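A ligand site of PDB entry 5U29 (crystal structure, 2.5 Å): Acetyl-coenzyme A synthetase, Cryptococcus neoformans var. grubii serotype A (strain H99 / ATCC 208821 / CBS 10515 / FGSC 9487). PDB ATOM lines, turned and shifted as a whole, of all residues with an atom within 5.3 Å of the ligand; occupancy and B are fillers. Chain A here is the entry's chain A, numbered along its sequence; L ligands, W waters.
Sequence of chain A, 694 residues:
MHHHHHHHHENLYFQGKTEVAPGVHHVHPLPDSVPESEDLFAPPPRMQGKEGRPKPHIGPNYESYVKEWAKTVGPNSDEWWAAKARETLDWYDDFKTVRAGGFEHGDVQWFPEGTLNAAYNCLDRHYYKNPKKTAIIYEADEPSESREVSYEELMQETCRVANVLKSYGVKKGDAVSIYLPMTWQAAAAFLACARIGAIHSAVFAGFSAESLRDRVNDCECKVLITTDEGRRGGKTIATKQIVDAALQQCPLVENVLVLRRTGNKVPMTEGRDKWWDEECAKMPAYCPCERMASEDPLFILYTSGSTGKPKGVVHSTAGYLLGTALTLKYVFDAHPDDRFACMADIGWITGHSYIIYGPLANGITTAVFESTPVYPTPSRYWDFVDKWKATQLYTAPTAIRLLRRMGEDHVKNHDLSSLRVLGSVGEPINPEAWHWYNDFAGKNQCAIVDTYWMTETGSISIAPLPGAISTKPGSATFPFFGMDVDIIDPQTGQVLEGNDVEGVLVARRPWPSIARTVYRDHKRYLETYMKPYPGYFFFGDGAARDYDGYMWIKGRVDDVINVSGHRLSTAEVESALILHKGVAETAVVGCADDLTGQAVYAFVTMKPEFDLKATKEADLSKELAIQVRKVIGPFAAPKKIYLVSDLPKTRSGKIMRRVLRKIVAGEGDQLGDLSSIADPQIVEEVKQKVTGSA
O7 of the ligand lies within hydrogen-bond range of OD2 of Asp 541, 2.5 Å away.
A nitrogen (N6) of the ligand sits at hydrogen-bond distance from the backbone carbonyl oxygen (O) of Thr 451 (2.7 Å).
O7 of the ligand sits at hydrogen-bond distance from NH1 of Arg 556 (2.8 Å).
NE1 of Trp 348 is in hydrogen-bond range of O3 of the ligand (2.9 Å).
An oxygen (O2) of the ligand lies within hydrogen-bond range of the backbone NH (N) of Thr 455, 3.0 Å away.
The side-chain hydroxyl of Thr 455 lies within hydrogen-bond range of an oxygen (O2) of the ligand (2.9 Å).
N of Gly 426 sits at hydrogen-bond distance from N3 of the ligand.
The side-chain carboxylate (OD1) of Asp 450 is in hydrogen-bond range of a nitrogen (N6) of the ligand.
N of Glu 427 lies close to N3 of the ligand (3.5 Å).
An oxygen (O7) of the ligand is in hydrogen-bond range of the side-chain sulfur of Met 454.
The guanidinium group (NH1) of Arg 556 is in salt-bridge range of the side-chain carboxylate (OD1) of Asp 541 (3.6 Å).
N of Thr 451 sits at hydrogen-bond distance from O of Ser 424 (2.9 Å).
The guanidinium group (NH1) of Arg 556 sits at hydrogen-bond distance from the backbone carbonyl oxygen (O) of Phe 539 (3.2 Å).
Ile 349 touches the ligand.
CG2 of Val 425 touches C1 of the ligand, at 3.7 Å.
Pro 428 touches the ligand.
Tyr 452 touches the ligand.
O of Trp 453 touches C1 of the ligand, at 3.4 Å.
Ile 553 touches the ligand.
Hydrophobic or aromatic side chains that line the ligand: Trp 348, Ile 349, Val 425, Pro 428, Tyr 452, Trp 453, Met 454 and Ile 553.
Of the 22 residues printed, 15 come within 4 Å of the ligand.
The nearest printed residue that does not touch the ligand is Thr 350 (4.1 Å).
Water W1 lies within hydrogen-bond range of OD1 of Asp 450 (2.6 Å), O of Glu 427 (2.7 Å), OG of Ser 424 (2.7 Å) and N6 of the ligand (3.4 Å).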
ATOM      1  N   TRP A 348      33.930  31.829   9.378  1.00  0.00           N
ATOM      2  CA  TRP A 348      32.943  31.333  10.324  1.00  0.00           C
ATOM      3  C   TRP A 348      33.656  31.019  11.626  1.00  0.00           C
ATOM      4  O   TRP A 348      34.820  30.583  11.618  1.00  0.00           O
ATOM      5  CB  TRP A 348      32.267  30.072   9.777  1.00  0.00           C
ATOM      6  CG  TRP A 348      31.063  29.529  10.544  1.00  0.00           C
ATOM      7  CD1 TRP A 348      30.279  30.205  11.442  1.00  0.00           C
ATOM      8  CD2 TRP A 348      30.499  28.219  10.429  1.00  0.00           C
ATOM      9  NE1 TRP A 348      29.271  29.399  11.894  1.00  0.00           N
ATOM     10  CE2 TRP A 348      29.390  28.159  11.288  1.00  0.00           C
ATOM     11  CE3 TRP A 348      30.827  27.085   9.664  1.00  0.00           C
ATOM     12  CZ2 TRP A 348      28.601  27.010  11.425  1.00  0.00           C
ATOM     13  CZ3 TRP A 348      30.046  25.935   9.808  1.00  0.00           C
ATOM     14  CH2 TRP A 348      28.939  25.910  10.681  1.00  0.00           C
ATOM     15  N   ILE A 349      32.948  31.206  12.745  1.00  0.00           N
ATOM     16  CA  ILE A 349      33.583  30.881  14.015  1.00  0.00           C
ATOM     17  C   ILE A 349      34.115  29.455  13.989  1.00  0.00           C
ATOM     18  O   ILE A 349      35.182  29.174  14.552  1.00  0.00           O
ATOM     19  CB  ILE A 349      32.632  31.118  15.214  1.00  0.00           C
ATOM     20  CG1 ILE A 349      33.417  30.956  16.511  1.00  0.00           C
ATOM     21  CG2 ILE A 349      31.485  30.096  15.242  1.00  0.00           C
ATOM     22  CD1 ILE A 349      34.470  32.060  16.698  1.00  0.00           C
ATOM     23  N   THR A 350      33.433  28.534  13.271  1.00  0.00           N
ATOM     24  CA  THR A 350      33.915  27.154  13.213  1.00  0.00           C
ATOM     25  C   THR A 350      35.340  27.082  12.674  1.00  0.00           C
ATOM     26  O   THR A 350      36.155  26.293  13.164  1.00  0.00           O
ATOM     27  CB  THR A 350      32.987  26.296  12.355  1.00  0.00           C
ATOM     28  OG1 THR A 350      31.640  26.409  12.832  1.00  0.00           O
ATOM     29  CG2 THR A 350      33.430  24.803  12.406  1.00  0.00           C
ATOM     30  N   SER A 424      29.226  17.323  13.298  1.00  0.00           N
ATOM     31  CA  SER A 424      28.195  18.096  12.629  1.00  0.00           C
ATOM     32  C   SER A 424      28.010  19.392  13.415  1.00  0.00           C
ATOM     33  O   SER A 424      27.912  19.345  14.646  1.00  0.00           O
ATOM     34  CB  SER A 424      26.896  17.264  12.565  1.00  0.00           C
ATOM     35  OG  SER A 424      25.814  17.976  11.988  1.00  0.00           O
ATOM     36  N   VAL A 425      27.985  20.538  12.724  1.00  0.00           N
ATOM     37  CA  VAL A 425      27.929  21.833  13.398  1.00  0.00           C
ATOM     38  C   VAL A 425      27.142  22.836  12.548  1.00  0.00           C
ATOM     39  O   VAL A 425      27.250  22.838  11.317  1.00  0.00           O
ATOM     40  CB  VAL A 425      29.334  22.383  13.703  1.00  0.00           C
ATOM     41  CG1 VAL A 425      30.164  22.366  12.438  1.00  0.00           C
ATOM     42  CG2 VAL A 425      29.243  23.791  14.249  1.00  0.00           C
ATOM     43  N   GLY A 426      26.361  23.698  13.210  1.00  0.00           N
ATOM     44  CA  GLY A 426      25.779  24.867  12.590  1.00  0.00           C
ATOM     45  C   GLY A 426      24.261  24.891  12.525  1.00  0.00           C
ATOM     46  O   GLY A 426      23.685  25.968  12.323  1.00  0.00           O
ATOM     47  N   GLU A 427      23.599  23.761  12.728  1.00  0.00           N
ATOM     48  CA  GLU A 427      22.146  23.637  12.627  1.00  0.00           C
ATOM     49  C   GLU A 427      21.744  22.262  13.152  1.00  0.00           C
ATOM     50  O   GLU A 427      22.594  21.362  13.245  1.00  0.00           O
ATOM     51  CB  GLU A 427      21.670  23.803  11.186  1.00  0.00           C
ATOM     52  CG  GLU A 427      20.944  25.066  10.922  1.00  0.00           C
ATOM     53  CD  GLU A 427      20.017  24.930   9.741  1.00  0.00           C
ATOM     54  OE1 GLU A 427      19.964  23.818   9.161  1.00  0.00           O
ATOM     55  OE2 GLU A 427      19.278  25.907   9.450  1.00  0.00           O
ATOM     56  N   PRO A 428      20.481  22.074  13.497  1.00  0.00           N
ATOM     57  CA  PRO A 428      20.057  20.722  13.874  1.00  0.00           C
ATOM     58  C   PRO A 428      20.283  19.789  12.703  1.00  0.00           C
ATOM     59  O   PRO A 428      20.016  20.145  11.552  1.00  0.00           O
ATOM     60  CB  PRO A 428      18.565  20.895  14.198  1.00  0.00           C
ATOM     61  CG  PRO A 428      18.391  22.379  14.499  1.00  0.00           C
ATOM     62  CD  PRO A 428      19.372  23.052  13.582  1.00  0.00           C
ATOM     63  N   ILE A 429      20.802  18.597  12.988  1.00  0.00           N
ATOM     64  CA  ILE A 429      20.966  17.573  11.953  1.00  0.00           C
ATOM     65  C   ILE A 429      19.791  16.624  12.049  1.00  0.00           C
ATOM     66  O   ILE A 429      19.556  16.007  13.095  1.00  0.00           O
ATOM     67  CB  ILE A 429      22.309  16.834  12.078  1.00  0.00           C
ATOM     68  CG1 ILE A 429      22.403  15.780  10.986  1.00  0.00           C
ATOM     69  CG2 ILE A 429      22.516  16.264  13.470  1.00  0.00           C
ATOM     70  CD1 ILE A 429      23.804  15.326  10.718  1.00  0.00           C
ATOM     71  N   ASP A 450      27.368  15.639  17.327  1.00  0.00           N
ATOM     72  CA  ASP A 450      26.560  16.801  17.000  1.00  0.00           C
ATOM     73  C   ASP A 450      26.938  17.913  17.974  1.00  0.00           C
ATOM     74  O   ASP A 450      26.636  17.818  19.169  1.00  0.00           O
ATOM     75  CB  ASP A 450      25.094  16.425  17.112  1.00  0.00           C
ATOM     76  CG  ASP A 450      24.157  17.526  16.720  1.00  0.00           C
ATOM     77  OD1 ASP A 450      24.614  18.516  16.129  1.00  0.00           O
ATOM     78  OD2 ASP A 450      22.938  17.378  16.964  1.00  0.00           O
ATOM     79  N   THR A 451      27.625  18.942  17.496  1.00  0.00           N
ATOM     80  CA  THR A 451      28.174  19.981  18.368  1.00  0.00           C
ATOM     81  C   THR A 451      27.323  21.241  18.288  1.00  0.00           C
ATOM     82  O   THR A 451      27.270  21.878  17.233  1.00  0.00           O
ATOM     83  CB  THR A 451      29.614  20.335  18.001  1.00  0.00           C
ATOM     84  OG1 THR A 451      29.620  21.041  16.764  1.00  0.00           O
ATOM     85  CG2 THR A 451      30.462  19.079  17.876  1.00  0.00           C
ATOM     86  N   TYR A 452      26.712  21.617  19.406  1.00  0.00           N
ATOM     87  CA  TYR A 452      25.926  22.841  19.500  1.00  0.00           C
ATOM     88  C   TYR A 452      26.782  23.936  20.137  1.00  0.00           C
ATOM     89  O   TYR A 452      27.381  23.718  21.201  1.00  0.00           O
ATOM     90  CB  TYR A 452      24.651  22.620  20.320  1.00  0.00           C
ATOM     91  CG  TYR A 452      23.980  23.931  20.672  1.00  0.00           C
ATOM     92  CD1 TYR A 452      23.175  24.582  19.736  1.00  0.00           C
ATOM     93  CD2 TYR A 452      24.171  24.536  21.905  1.00  0.00           C
ATOM     94  CE1 TYR A 452      22.571  25.793  20.034  1.00  0.00           C
ATOM     95  CE2 TYR A 452      23.572  25.737  22.212  1.00  0.00           C
ATOM     96  CZ  TYR A 452      22.788  26.359  21.265  1.00  0.00           C
ATOM     97  OH  TYR A 452      22.203  27.557  21.570  1.00  0.00           O
ATOM     98  N   TRP A 453      26.879  25.093  19.472  1.00  0.00           N
ATOM     99  CA  TRP A 453      27.544  26.275  20.029  1.00  0.00           C
ATOM    100  C   TRP A 453      27.280  27.473  19.113  1.00  0.00           C
ATOM    101  O   TRP A 453      26.563  27.362  18.103  1.00  0.00           O
ATOM    102  CB  TRP A 453      29.061  26.076  20.246  1.00  0.00           C
ATOM    103  CG  TRP A 453      29.880  25.685  19.031  1.00  0.00           C
ATOM    104  CD1 TRP A 453      29.716  24.573  18.255  1.00  0.00           C
ATOM    105  CD2 TRP A 453      30.975  26.405  18.468  1.00  0.00           C
ATOM    106  NE1 TRP A 453      30.657  24.562  17.251  1.00  0.00           N
ATOM    107  CE2 TRP A 453      31.443  25.674  17.355  1.00  0.00           C
ATOM    108  CE3 TRP A 453      31.621  27.589  18.795  1.00  0.00           C
ATOM    109  CZ2 TRP A 453      32.508  26.105  16.564  1.00  0.00           C
ATOM    110  CZ3 TRP A 453      32.678  28.008  18.029  1.00  0.00           C
ATOM    111  CH2 TRP A 453      33.107  27.264  16.916  1.00  0.00           C
ATOM    112  N   MET A 454      27.796  28.631  19.520  1.00  0.00           N
ATOM    113  CA  MET A 454      27.640  29.863  18.757  1.00  0.00           C
ATOM    114  C   MET A 454      28.941  30.657  18.705  1.00  0.00           C
ATOM    115  O   MET A 454      29.873  30.435  19.485  1.00  0.00           O
ATOM    116  CB  MET A 454      26.542  30.768  19.351  1.00  0.00           C
ATOM    117  CG  MET A 454      25.451  30.060  20.100  1.00  0.00           C
ATOM    118  SD  MET A 454      24.159  31.208  20.561  1.00  0.00           S
ATOM    119  CE  MET A 454      25.000  32.327  21.646  1.00  0.00           C
ATOM    120  N   THR A 455      28.971  31.628  17.767  1.00  0.00           N
ATOM    121  CA  THR A 455      30.073  32.567  17.697  1.00  0.00           C
ATOM    122  C   THR A 455      30.369  33.177  19.053  1.00  0.00           C
ATOM    123  O   THR A 455      31.533  33.291  19.465  1.00  0.00           O
ATOM    124  CB  THR A 455      29.745  33.679  16.712  1.00  0.00           C
ATOM    125  OG1 THR A 455      29.639  33.120  15.392  1.00  0.00           O
ATOM    126  CG2 THR A 455      30.826  34.764  16.753  1.00  0.00           C
ATOM    127  N   GLU A 456      29.305  33.538  19.776  1.00  0.00           N
ATOM    128  CA  GLU A 456      29.422  34.144  21.085  1.00  0.00           C
ATOM    129  C   GLU A 456      29.936  33.195  22.179  1.00  0.00           C
ATOM    130  O   GLU A 456      30.391  33.694  23.210  1.00  0.00           O
ATOM    131  CB  GLU A 456      28.069  34.673  21.535  1.00  0.00           C
ATOM    132  CG  GLU A 456      27.513  35.784  20.690  1.00  0.00           C
ATOM    133  CD  GLU A 456      26.723  35.280  19.501  1.00  0.00           C
ATOM    134  OE1 GLU A 456      26.920  34.124  19.057  1.00  0.00           O
ATOM    135  OE2 GLU A 456      25.890  36.060  19.001  1.00  0.00           O
ATOM    136  N   PHE A 539      21.076  32.072  24.813  1.00  0.00           N
ATOM    137  CA  PHE A 539      21.558  31.618  23.502  1.00  0.00           C
ATOM    138  C   PHE A 539      20.666  32.078  22.348  1.00  0.00           C
ATOM    139  O   PHE A 539      21.144  32.239  21.239  1.00  0.00           O
ATOM    140  CB  PHE A 539      21.632  30.087  23.450  1.00  0.00           C
ATOM    141  CG  PHE A 539      22.634  29.466  24.383  1.00  0.00           C
ATOM    142  CD1 PHE A 539      22.280  29.144  25.682  1.00  0.00           C
ATOM    143  CD2 PHE A 539      23.913  29.175  23.937  1.00  0.00           C
ATOM    144  CE1 PHE A 539      23.205  28.564  26.537  1.00  0.00           C
ATOM    145  CE2 PHE A 539      24.844  28.591  24.784  1.00  0.00           C
ATOM    146  CZ  PHE A 539      24.494  28.289  26.079  1.00  0.00           C
ATOM    147  N   ASP A 541      18.167  30.031  21.353  1.00  0.00           N
ATOM    148  CA  ASP A 541      17.661  28.791  20.787  1.00  0.00           C
ATOM    149  C   ASP A 541      16.599  28.177  21.695  1.00  0.00           C
ATOM    150  O   ASP A 541      16.681  28.238  22.931  1.00  0.00           O
ATOM    151  CB  ASP A 541      18.789  27.781  20.581  1.00  0.00           C
ATOM    152  CG  ASP A 541      19.740  28.191  19.454  1.00  0.00           C
ATOM    153  OD1 ASP A 541      19.258  28.438  18.310  1.00  0.00           O
ATOM    154  OD2 ASP A 541      20.964  28.251  19.693  1.00  0.00           O
ATOM    155  N   ILE A 553      18.310  20.544  20.666  1.00  0.00           N
ATOM    156  CA  ILE A 553      18.219  21.913  20.193  1.00  0.00           C
ATOM    157  C   ILE A 553      17.128  21.934  19.126  1.00  0.00           C
ATOM    158  O   ILE A 553      17.228  21.252  18.102  1.00  0.00           O
ATOM    159  CB  ILE A 553      19.574  22.402  19.650  1.00  0.00           C
ATOM    160  CG1 ILE A 553      20.662  22.238  20.733  1.00  0.00           C
ATOM    161  CG2 ILE A 553      19.527  23.870  19.239  1.00  0.00           C
ATOM    162  CD1 ILE A 553      20.335  22.966  22.054  1.00  0.00           C
ATOM    163  N   GLY A 555      15.791  24.712  17.446  1.00  0.00           N
ATOM    164  CA  GLY A 555      15.885  25.735  16.431  1.00  0.00           C
ATOM    165  C   GLY A 555      15.865  27.112  17.046  1.00  0.00           C
ATOM    166  O   GLY A 555      15.702  27.285  18.256  1.00  0.00           O
ATOM    167  N   ARG A 556      16.041  28.121  16.183  1.00  0.00           N
ATOM    168  CA  ARG A 556      16.053  29.505  16.632  1.00  0.00           C
ATOM    169  C   ARG A 556      14.678  29.874  17.184  1.00  0.00           C
ATOM    170  O   ARG A 556      13.653  29.551  16.593  1.00  0.00           O
ATOM    171  CB  ARG A 556      16.442  30.465  15.489  1.00  0.00           C
ATOM    172  CG  ARG A 556      17.883  30.399  14.946  1.00  0.00           C
ATOM    173  CD  ARG A 556      18.923  30.669  16.041  1.00  0.00           C
ATOM    174  NE  ARG A 556      18.945  32.069  16.479  1.00  0.00           N
ATOM    175  CZ  ARG A 556      19.727  32.556  17.454  1.00  0.00           C
ATOM    176  NH1 ARG A 556      20.577  31.766  18.107  1.00  0.00           N
ATOM    177  NH2 ARG A 556      19.645  33.837  17.777  1.00  0.00           N
ATOM    178  N   SER A 652      27.850  29.548   7.074  1.00  0.00           N
ATOM    179  CA  SER A 652      27.747  29.404   8.515  1.00  0.00           C
ATOM    180  C   SER A 652      26.799  28.263   8.897  1.00  0.00           C
ATOM    181  O   SER A 652      26.176  28.272   9.968  1.00  0.00           O
ATOM    182  CB  SER A 652      27.317  30.738   9.143  1.00  0.00           C
ATOM    183  OG  SER A 652      25.963  31.063   8.856  1.00  0.00           O
HETATM  184  C1  LIG L   1      28.716  27.240  15.519  1.00  0.00           C
HETATM  185  C2  LIG L   1      27.785  28.239  14.878  1.00  0.00           C
HETATM  186  C3  LIG L   1      25.013  29.688  16.129  1.00  0.00           C
HETATM  187  C4  LIG L   1      23.572  29.217  15.952  1.00  0.00           C
HETATM  188  C5  LIG L   1      22.974  28.592  17.208  1.00  0.00           C
HETATM  189  C6  LIG L   1      21.989  27.604  16.639  1.00  0.00           C
HETATM  190  C7  LIG L   1      22.619  27.154  15.352  1.00  0.00           C
HETATM  191  C8  LIG L   1      24.716  25.792  15.541  1.00  0.00           C
HETATM  192  C9  LIG L   1      23.928  23.828  16.012  1.00  0.00           C
HETATM  193  C10 LIG L   1      22.867  24.712  15.877  1.00  0.00           C
HETATM  194  C11 LIG L   1      21.377  22.986  16.350  1.00  0.00           C
HETATM  195  C12 LIG L   1      23.677  22.485  16.321  1.00  0.00           C
HETATM  196  N1  LIG L   1      27.899  29.499  15.339  1.00  0.00           N
HETATM  197  N2  LIG L   1      23.383  25.906  15.586  1.00  0.00           N
HETATM  198  N3  LIG L   1      25.066  24.514  15.792  1.00  0.00           N
HETATM  199  N4  LIG L   1      21.601  24.273  16.042  1.00  0.00           N
HETATM  200  N5  LIG L   1      22.388  22.103  16.483  1.00  0.00           N
HETATM  201  N6  LIG L   1      24.701  21.598  16.453  1.00  0.00           N
HETATM  202  O1  LIG L   1      26.962  27.918  13.990  1.00  0.00           O
HETATM  203  O2  LIG L   1      27.102  31.823  15.457  1.00  0.00           O
HETATM  204  O3  LIG L   1      27.193  30.735  13.317  1.00  0.00           O
HETATM  205  O4  LIG L   1      25.466  30.109  14.854  1.00  0.00           O
HETATM  206  O5  LIG L   1      23.533  28.191  14.944  1.00  0.00           O
HETATM  207  O6  LIG L   1      20.810  28.318  16.293  1.00  0.00           O
HETATM  208  O7  LIG L   1      22.317  29.551  18.038  1.00  0.00           O
HETATM  209  S1  LIG L   1      26.914  30.600  14.721  1.00  0.00           S
HETATM  210  O   HOH W   1      24.433  19.504  13.766  1.00  0.00           O
HETATM  211  O   HOH W   2      19.256  26.255  15.132  1.00  0.00           O
HETATM  212  O   HOH W   3      25.013  28.587  12.417  1.00  0.00           O
